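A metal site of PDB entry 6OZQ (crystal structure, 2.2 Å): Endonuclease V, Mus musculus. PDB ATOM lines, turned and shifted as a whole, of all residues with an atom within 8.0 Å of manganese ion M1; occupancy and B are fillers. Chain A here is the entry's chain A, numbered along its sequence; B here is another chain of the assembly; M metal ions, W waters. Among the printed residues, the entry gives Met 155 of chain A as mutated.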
ATOM      1  N   VAL A  51     -12.669  28.997 -17.791  1.00  0.00           N
ATOM      2  CA  VAL A  51     -11.559  29.951 -17.827  1.00  0.00           C
ATOM      3  C   VAL A  51     -10.289  29.294 -17.329  1.00  0.00           C
ATOM      4  O   VAL A  51     -10.310  28.316 -16.574  1.00  0.00           O
ATOM      5  CB  VAL A  51     -11.837  31.229 -17.001  1.00  0.00           C
ATOM      6  CG1 VAL A  51     -12.996  31.997 -17.576  1.00  0.00           C
ATOM      7  CG2 VAL A  51     -12.062  30.875 -15.531  1.00  0.00           C
ATOM      8  N   ASP A  52      -9.162  29.891 -17.705  1.00  0.00           N
ATOM      9  CA  ASP A  52      -7.857  29.452 -17.213  1.00  0.00           C
ATOM     10  C   ASP A  52      -6.863  30.603 -17.340  1.00  0.00           C
ATOM     11  O   ASP A  52      -6.942  31.403 -18.274  1.00  0.00           O
ATOM     12  CB  ASP A  52      -7.324  28.242 -17.988  1.00  0.00           C
ATOM     13  CG  ASP A  52      -5.900  27.831 -17.545  1.00  0.00           C
ATOM     14  OD1 ASP A  52      -5.635  27.776 -16.316  1.00  0.00           O
ATOM     15  OD2 ASP A  52      -5.045  27.565 -18.411  1.00  0.00           O
ATOM     16  N   VAL A  53      -5.930  30.660 -16.401  1.00  0.00           N
ATOM     17  CA  VAL A  53      -4.799  31.572 -16.472  1.00  0.00           C
ATOM     18  C   VAL A  53      -3.542  30.767 -16.159  1.00  0.00           C
ATOM     19  O   VAL A  53      -3.304  30.413 -14.998  1.00  0.00           O
ATOM     20  CB  VAL A  53      -4.936  32.758 -15.517  1.00  0.00           C
ATOM     21  CG1 VAL A  53      -3.733  33.670 -15.701  1.00  0.00           C
ATOM     22  CG2 VAL A  53      -6.224  33.509 -15.771  1.00  0.00           C
ATOM     23  N   SER A  54      -2.725  30.511 -17.185  1.00  0.00           N
ATOM     24  CA  SER A  54      -1.496  29.748 -17.057  1.00  0.00           C
ATOM     25  C   SER A  54      -0.297  30.662 -17.220  1.00  0.00           C
ATOM     26  O   SER A  54      -0.400  31.780 -17.718  1.00  0.00           O
ATOM     27  CB  SER A  54      -1.439  28.634 -18.101  1.00  0.00           C
ATOM     28  OG  SER A  54      -2.449  27.670 -17.874  1.00  0.00           O
ATOM     29  N   SER A  66      -7.244  32.323 -20.769  1.00  0.00           N
ATOM     30  CA  SER A  66      -8.067  31.693 -21.792  1.00  0.00           C
ATOM     31  C   SER A  66      -9.523  31.601 -21.340  1.00  0.00           C
ATOM     32  O   SER A  66      -9.808  31.328 -20.173  1.00  0.00           O
ATOM     33  CB  SER A  66      -7.531  30.286 -22.129  1.00  0.00           C
ATOM     34  OG  SER A  66      -6.313  30.337 -22.844  1.00  0.00           O
ATOM     35  N   GLU A 100      -5.712  37.463 -11.053  1.00  0.00           N
ATOM     36  CA  GLU A 100      -6.231  37.085 -12.368  1.00  0.00           C
ATOM     37  C   GLU A 100      -7.587  37.649 -12.753  1.00  0.00           C
ATOM     38  O   GLU A 100      -7.884  37.698 -13.956  1.00  0.00           O
ATOM     39  CB  GLU A 100      -6.313  35.556 -12.501  1.00  0.00           C
ATOM     40  CG  GLU A 100      -6.942  34.875 -11.332  1.00  0.00           C
ATOM     41  CD  GLU A 100      -6.987  33.356 -11.503  1.00  0.00           C
ATOM     42  OE1 GLU A 100      -8.047  32.769 -11.201  1.00  0.00           O
ATOM     43  OE2 GLU A 100      -5.999  32.757 -11.958  1.00  0.00           O
ATOM     44  N   VAL A 125     -15.109  27.854 -13.015  1.00  0.00           N
ATOM     45  CA  VAL A 125     -13.844  28.518 -12.683  1.00  0.00           C
ATOM     46  C   VAL A 125     -12.937  27.532 -11.966  1.00  0.00           C
ATOM     47  O   VAL A 125     -13.408  26.739 -11.134  1.00  0.00           O
ATOM     48  CB  VAL A 125     -14.125  29.764 -11.820  1.00  0.00           C
ATOM     49  CG1 VAL A 125     -12.855  30.561 -11.551  1.00  0.00           C
ATOM     50  CG2 VAL A 125     -15.159  30.648 -12.519  1.00  0.00           C
ATOM     51  N   ASP A 126     -11.644  27.530 -12.325  1.00  0.00           N
ATOM     52  CA  ASP A 126     -10.665  26.690 -11.634  1.00  0.00           C
ATOM     53  C   ASP A 126     -10.183  27.409 -10.380  1.00  0.00           C
ATOM     54  O   ASP A 126      -9.198  28.138 -10.384  1.00  0.00           O
ATOM     55  CB  ASP A 126      -9.493  26.322 -12.558  1.00  0.00           C
ATOM     56  CG  ASP A 126      -8.908  27.524 -13.300  1.00  0.00           C
ATOM     57  OD1 ASP A 126      -9.597  28.566 -13.383  1.00  0.00           O
ATOM     58  OD2 ASP A 126      -7.773  27.421 -13.807  1.00  0.00           O
ATOM     59  N   GLY A 127     -10.879  27.160  -9.282  1.00  0.00           N
ATOM     60  CA  GLY A 127     -10.648  27.804  -8.010  1.00  0.00           C
ATOM     61  C   GLY A 127     -11.960  27.833  -7.253  1.00  0.00           C
ATOM     62  O   GLY A 127     -13.034  27.635  -7.801  1.00  0.00           O
ATOM     63  N   VAL A 153     -14.522  25.196  -8.977  1.00  0.00           N
ATOM     64  CA  VAL A 153     -14.026  23.830  -9.045  1.00  0.00           C
ATOM     65  C   VAL A 153     -12.545  23.848  -8.674  1.00  0.00           C
ATOM     66  O   VAL A 153     -11.736  24.455  -9.392  1.00  0.00           O
ATOM     67  CB  VAL A 153     -14.210  23.201 -10.436  1.00  0.00           C
ATOM     68  CG1 VAL A 153     -13.739  21.729 -10.386  1.00  0.00           C
ATOM     69  CG2 VAL A 153     -15.653  23.285 -10.889  1.00  0.00           C
ATOM     70  N   MET A 155      -9.007  21.467  -7.292  1.00  0.00           N
ATOM     71  CA  MET A 155      -8.338  20.161  -7.325  1.00  0.00           C
ATOM     72  C   MET A 155      -7.816  19.709  -5.968  1.00  0.00           C
ATOM     73  O   MET A 155      -7.549  18.515  -5.803  1.00  0.00           O
ATOM     74  CB  MET A 155      -7.141  20.195  -8.287  1.00  0.00           C
ATOM     75  CG  MET A 155      -7.471  20.568  -9.710  1.00  0.00           C
ATOM     76  SD  MET A 155      -8.915  19.655 -10.285  1.00  0.00           S
ATOM     77  CE  MET A 155      -9.914  20.974 -10.994  1.00  0.00           C
ATOM     78  N   ILE A 232     -11.177  16.337 -14.915  1.00  0.00           N
ATOM     79  CA  ILE A 232     -11.353  17.781 -15.003  1.00  0.00           C
ATOM     80  C   ILE A 232     -12.561  18.078 -15.894  1.00  0.00           C
ATOM     81  O   ILE A 232     -12.629  17.546 -17.013  1.00  0.00           O
ATOM     82  CB  ILE A 232     -10.095  18.435 -15.563  1.00  0.00           C
ATOM     83  CG1 ILE A 232      -8.873  17.930 -14.816  1.00  0.00           C
ATOM     84  CG2 ILE A 232     -10.178  19.964 -15.515  1.00  0.00           C
ATOM     85  CD1 ILE A 232      -8.962  18.120 -13.342  1.00  0.00           C
ATOM     86  N   PRO A 235     -15.098  22.156 -19.738  1.00  0.00           N
ATOM     87  CA  PRO A 235     -14.795  23.593 -19.976  1.00  0.00           C
ATOM     88  C   PRO A 235     -13.459  24.050 -19.369  1.00  0.00           C
ATOM     89  O   PRO A 235     -12.698  24.760 -20.046  1.00  0.00           O
ATOM     90  CB  PRO A 235     -15.984  24.311 -19.329  1.00  0.00           C
ATOM     91  CG  PRO A 235     -17.077  23.282 -19.291  1.00  0.00           C
ATOM     92  CD  PRO A 235     -16.378  21.986 -19.031  1.00  0.00           C
ATOM     93  N   ILE A 236     -13.177  23.684 -18.126  1.00  0.00           N
ATOM     94  CA  ILE A 236     -11.894  24.011 -17.489  1.00  0.00           C
ATOM     95  C   ILE A 236     -10.748  23.310 -18.209  1.00  0.00           C
ATOM     96  O   ILE A 236      -9.651  23.868 -18.388  1.00  0.00           O
ATOM     97  CB  ILE A 236     -11.914  23.637 -16.002  1.00  0.00           C
ATOM     98  CG1 ILE A 236     -12.724  24.643 -15.190  1.00  0.00           C
ATOM     99  CG2 ILE A 236     -10.485  23.495 -15.421  1.00  0.00           C
ATOM    100  CD1 ILE A 236     -13.071  24.130 -13.808  1.00  0.00           C
ATOM    101  N   ARG A 237     -10.972  22.069 -18.621  1.00  0.00           N
ATOM    102  CA  ARG A 237      -9.935  21.278 -19.273  1.00  0.00           C
ATOM    103  C   ARG A 237      -9.581  21.860 -20.634  1.00  0.00           C
ATOM    104  O   ARG A 237      -8.398  21.959 -20.984  1.00  0.00           O
ATOM    105  CB  ARG A 237     -10.421  19.832 -19.371  1.00  0.00           C
ATOM    106  CG  ARG A 237      -9.451  18.898 -20.009  1.00  0.00           C
ATOM    107  CD  ARG A 237      -9.946  17.451 -20.017  1.00  0.00           C
ATOM    108  NE  ARG A 237      -9.001  16.677 -20.832  1.00  0.00           N
ATOM    109  CZ  ARG A 237      -9.216  16.367 -22.109  1.00  0.00           C
ATOM    110  NH1 ARG A 237     -10.351  16.716 -22.695  1.00  0.00           N
ATOM    111  NH2 ARG A 237      -8.288  15.709 -22.790  1.00  0.00           N
ATOM    112  N   ALA A 239      -9.953  24.983 -21.640  1.00  0.00           N
ATOM    113  CA  ALA A 239      -9.251  26.239 -21.413  1.00  0.00           C
ATOM    114  C   ALA A 239      -7.795  26.001 -21.020  1.00  0.00           C
ATOM    115  O   ALA A 239      -6.899  26.746 -21.450  1.00  0.00           O
ATOM    116  CB  ALA A 239      -9.981  27.055 -20.335  1.00  0.00           C
ATOM    117  N   ASP A 240      -7.548  25.005 -20.162  1.00  0.00           N
ATOM    118  CA  ASP A 240      -6.187  24.579 -19.832  1.00  0.00           C
ATOM    119  C   ASP A 240      -5.409  24.177 -21.075  1.00  0.00           C
ATOM    120  O   ASP A 240      -4.239  24.527 -21.245  1.00  0.00           O
ATOM    121  CB  ASP A 240      -6.204  23.393 -18.867  1.00  0.00           C
ATOM    122  CG  ASP A 240      -6.392  23.797 -17.426  1.00  0.00           C
ATOM    123  OD1 ASP A 240      -5.974  24.906 -17.056  1.00  0.00           O
ATOM    124  OD2 ASP A 240      -6.958  22.971 -16.654  1.00  0.00           O
ATOM    125  N   ILE A 241      -6.010  23.329 -21.910  1.00  0.00           N
ATOM    126  CA  ILE A 241      -5.304  22.839 -23.088  1.00  0.00           C
ATOM    127  C   ILE A 241      -4.954  24.002 -24.005  1.00  0.00           C
ATOM    128  O   ILE A 241      -3.819  24.105 -24.488  1.00  0.00           O
ATOM    129  CB  ILE A 241      -6.146  21.792 -23.833  1.00  0.00           C
ATOM    130  CG1 ILE A 241      -6.203  20.511 -23.010  1.00  0.00           C
ATOM    131  CG2 ILE A 241      -5.547  21.520 -25.201  1.00  0.00           C
ATOM    132  CD1 ILE A 241      -7.249  19.530 -23.517  1.00  0.00           C
ATOM    133  N   SER A 243      -4.651  27.223 -23.410  1.00  0.00           N
ATOM    134  CA  SER A 243      -3.704  28.204 -22.923  1.00  0.00           C
ATOM    135  C   SER A 243      -2.269  27.692 -23.064  1.00  0.00           C
ATOM    136  O   SER A 243      -1.382  28.446 -23.487  1.00  0.00           O
ATOM    137  CB  SER A 243      -4.015  28.575 -21.475  1.00  0.00           C
ATOM    138  OG  SER A 243      -3.273  27.767 -20.584  1.00  0.00           O
ATOM    139  P     A B  11      -6.244  24.297  -7.006  1.00  0.00           P
ATOM    140  OP1   A B  11      -7.237  23.627  -7.884  1.00  0.00           O
ATOM    141  OP2   A B  11      -5.043  23.543  -6.583  1.00  0.00           O
ATOM    142  O5'   A B  11      -5.792  25.591  -7.810  1.00  0.00           O
ATOM    143  C5'   A B  11      -6.725  26.365  -8.548  1.00  0.00           C
ATOM    144  C4'   A B  11      -6.051  27.577  -9.152  1.00  0.00           C
ATOM    145  O4'   A B  11      -5.391  28.329  -8.095  1.00  0.00           O
ATOM    146  C3'   A B  11      -4.945  27.297 -10.139  1.00  0.00           C
ATOM    147  O3'   A B  11      -5.403  26.973 -11.449  1.00  0.00           O
ATOM    148  C2'   A B  11      -4.107  28.565 -10.075  1.00  0.00           C
ATOM    149  O2'   A B  11      -4.691  29.629 -10.815  1.00  0.00           O
ATOM    150  C1'   A B  11      -4.197  28.891  -8.588  1.00  0.00           C
ATOM    151  N9    A B  11      -3.088  28.295  -7.807  1.00  0.00           N
ATOM    152  C8    A B  11      -3.141  27.240  -6.936  1.00  0.00           C
ATOM    153  N7    A B  11      -1.988  26.959  -6.372  1.00  0.00           N
ATOM    154  C5    A B  11      -1.138  27.900  -6.906  1.00  0.00           C
ATOM    155  C6    A B  11       0.233  28.157  -6.714  1.00  0.00           C
ATOM    156  N6    A B  11       0.995  27.445  -5.892  1.00  0.00           N
ATOM    157  N1    A B  11       0.788  29.174  -7.400  1.00  0.00           N
ATOM    158  C2    A B  11       0.015  29.908  -8.222  1.00  0.00           C
ATOM    159  N3    A B  11      -1.282  29.764  -8.480  1.00  0.00           N
ATOM    160  C4    A B  11      -1.798  28.741  -7.781  1.00  0.00           C
ATOM    161  P     U B  12      -4.626  25.865 -12.300  1.00  0.00           P
ATOM    162  OP1   U B  12      -5.215  25.727 -13.662  1.00  0.00           O
ATOM    163  OP2   U B  12      -4.472  24.662 -11.462  1.00  0.00           O
ATOM    164  O5'   U B  12      -3.193  26.498 -12.466  1.00  0.00           O
ATOM    165  C5'   U B  12      -2.997  27.632 -13.277  1.00  0.00           C
ATOM    166  C4'   U B  12      -1.596  28.139 -13.139  1.00  0.00           C
ATOM    167  O4'   U B  12      -1.311  28.439 -11.737  1.00  0.00           O
ATOM    168  C3'   U B  12      -0.501  27.154 -13.535  1.00  0.00           C
ATOM    169  O3'   U B  12      -0.275  27.081 -14.934  1.00  0.00           O
ATOM    170  C2'   U B  12       0.694  27.682 -12.759  1.00  0.00           C
ATOM    171  O2'   U B  12       1.186  28.839 -13.400  1.00  0.00           O
ATOM    172  C1'   U B  12       0.038  28.103 -11.450  1.00  0.00           C
ATOM    173  N1    U B  12       0.066  26.997 -10.446  1.00  0.00           N
ATOM    174  C2    U B  12       1.252  26.762  -9.772  1.00  0.00           C
ATOM    175  O2    U B  12       2.278  27.399  -9.965  1.00  0.00           O
ATOM    176  N3    U B  12       1.227  25.731  -8.869  1.00  0.00           N
ATOM    177  C4    U B  12       0.155  24.924  -8.561  1.00  0.00           C
ATOM    178  O4    U B  12       0.283  24.050  -7.714  1.00  0.00           O
ATOM    179  C5    U B  12      -1.050  25.208  -9.291  1.00  0.00           C
ATOM    180  C6    U B  12      -1.041  26.212 -10.192  1.00  0.00           C
ATOM    181  P     A B  13       0.133  25.676 -15.614  1.00  0.00           P
ATOM    182  OP1   A B  13      -0.026  25.829 -17.080  1.00  0.00           O
ATOM    183  OP2   A B  13      -0.553  24.570 -14.915  1.00  0.00           O
ATOM    184  O5'   A B  13       1.695  25.538 -15.248  1.00  0.00           O
ATOM    185  C5'   A B  13       2.636  26.548 -15.573  1.00  0.00           C
ATOM    186  C4'   A B  13       3.929  26.383 -14.801  1.00  0.00           C
ATOM    187  O4'   A B  13       3.701  26.572 -13.379  1.00  0.00           O
ATOM    188  C3'   A B  13       4.558  25.005 -14.877  1.00  0.00           C
ATOM    189  O3'   A B  13       5.261  24.760 -16.083  1.00  0.00           O
ATOM    190  C2'   A B  13       5.416  24.968 -13.625  1.00  0.00           C
ATOM    191  O2'   A B  13       6.582  25.777 -13.782  1.00  0.00           O
ATOM    192  C1'   A B  13       4.491  25.663 -12.630  1.00  0.00           C
ATOM    193  N9    A B  13       3.603  24.687 -11.956  1.00  0.00           N
ATOM    194  C8    A B  13       2.297  24.385 -12.283  1.00  0.00           C
ATOM    195  N7    A B  13       1.748  23.489 -11.500  1.00  0.00           N
ATOM    196  C5    A B  13       2.743  23.161 -10.611  1.00  0.00           C
ATOM    197  C6    A B  13       2.787  22.253  -9.525  1.00  0.00           C
ATOM    198  N6    A B  13       1.744  21.498  -9.176  1.00  0.00           N
ATOM    199  N1    A B  13       3.931  22.148  -8.823  1.00  0.00           N
ATOM    200  C2    A B  13       4.975  22.918  -9.191  1.00  0.00           C
ATOM    201  N3    A B  13       5.068  23.795 -10.188  1.00  0.00           N
ATOM    202  C4    A B  13       3.900  23.886 -10.871  1.00  0.00           C
HETATM  203 MN    MN M   1      -6.755  25.907 -15.278  1.00  0.00          MN
HETATM  204 MN    MN M   2      -2.144  23.193 -15.266  1.00  0.00          MN
HETATM  205  O   HOH W   1      -8.791  26.024 -16.488  1.00  0.00           O
HETATM  206  O   HOH W   2      -7.280  23.740 -14.199  1.00  0.00           O
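O of Asp 240 is in hydrogen-bond range of OG of Ser 243 (3.4 Å). OD2 of Asp 52 sits at hydrogen-bond distance from OG of Ser 54 (2.7 Å). The side-chain carboxylate (OD2) of Asp 52 lies within hydrogen-bond range of the side-chain hydroxyl (OG) of Ser 243 (2.8 Å). The backbone carbonyl oxygen (O) of Asp 52 is in hydrogen-bond range of the backbone NH (N) of Ser 66, at 2.7 Å.
The nearest printed residue that does not touch manganese ion M1 is A 11 of chain B (4.2 Å).
Manganese ion M1 is bound by the side-chain carboxylate (OD1) of Asp 240, 2.2 Å away. Manganese ion M1 is bound by OP1 of U 12 of chain B, at 2.2 Å. OD2 of Asp 126 binds manganese ion M1 (2.3 Å). Manganese ion M1 is bound by water W1, at 2.4 Å. OD1 of Asp 52 is bound to manganese ion M1. Manganese ion M1 is bound by water W2, 2.5 Å away. Manganese ion M1 has six donor atoms within binding distance.
Water W1 bridges O of Val 51 and O of Ile 236.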
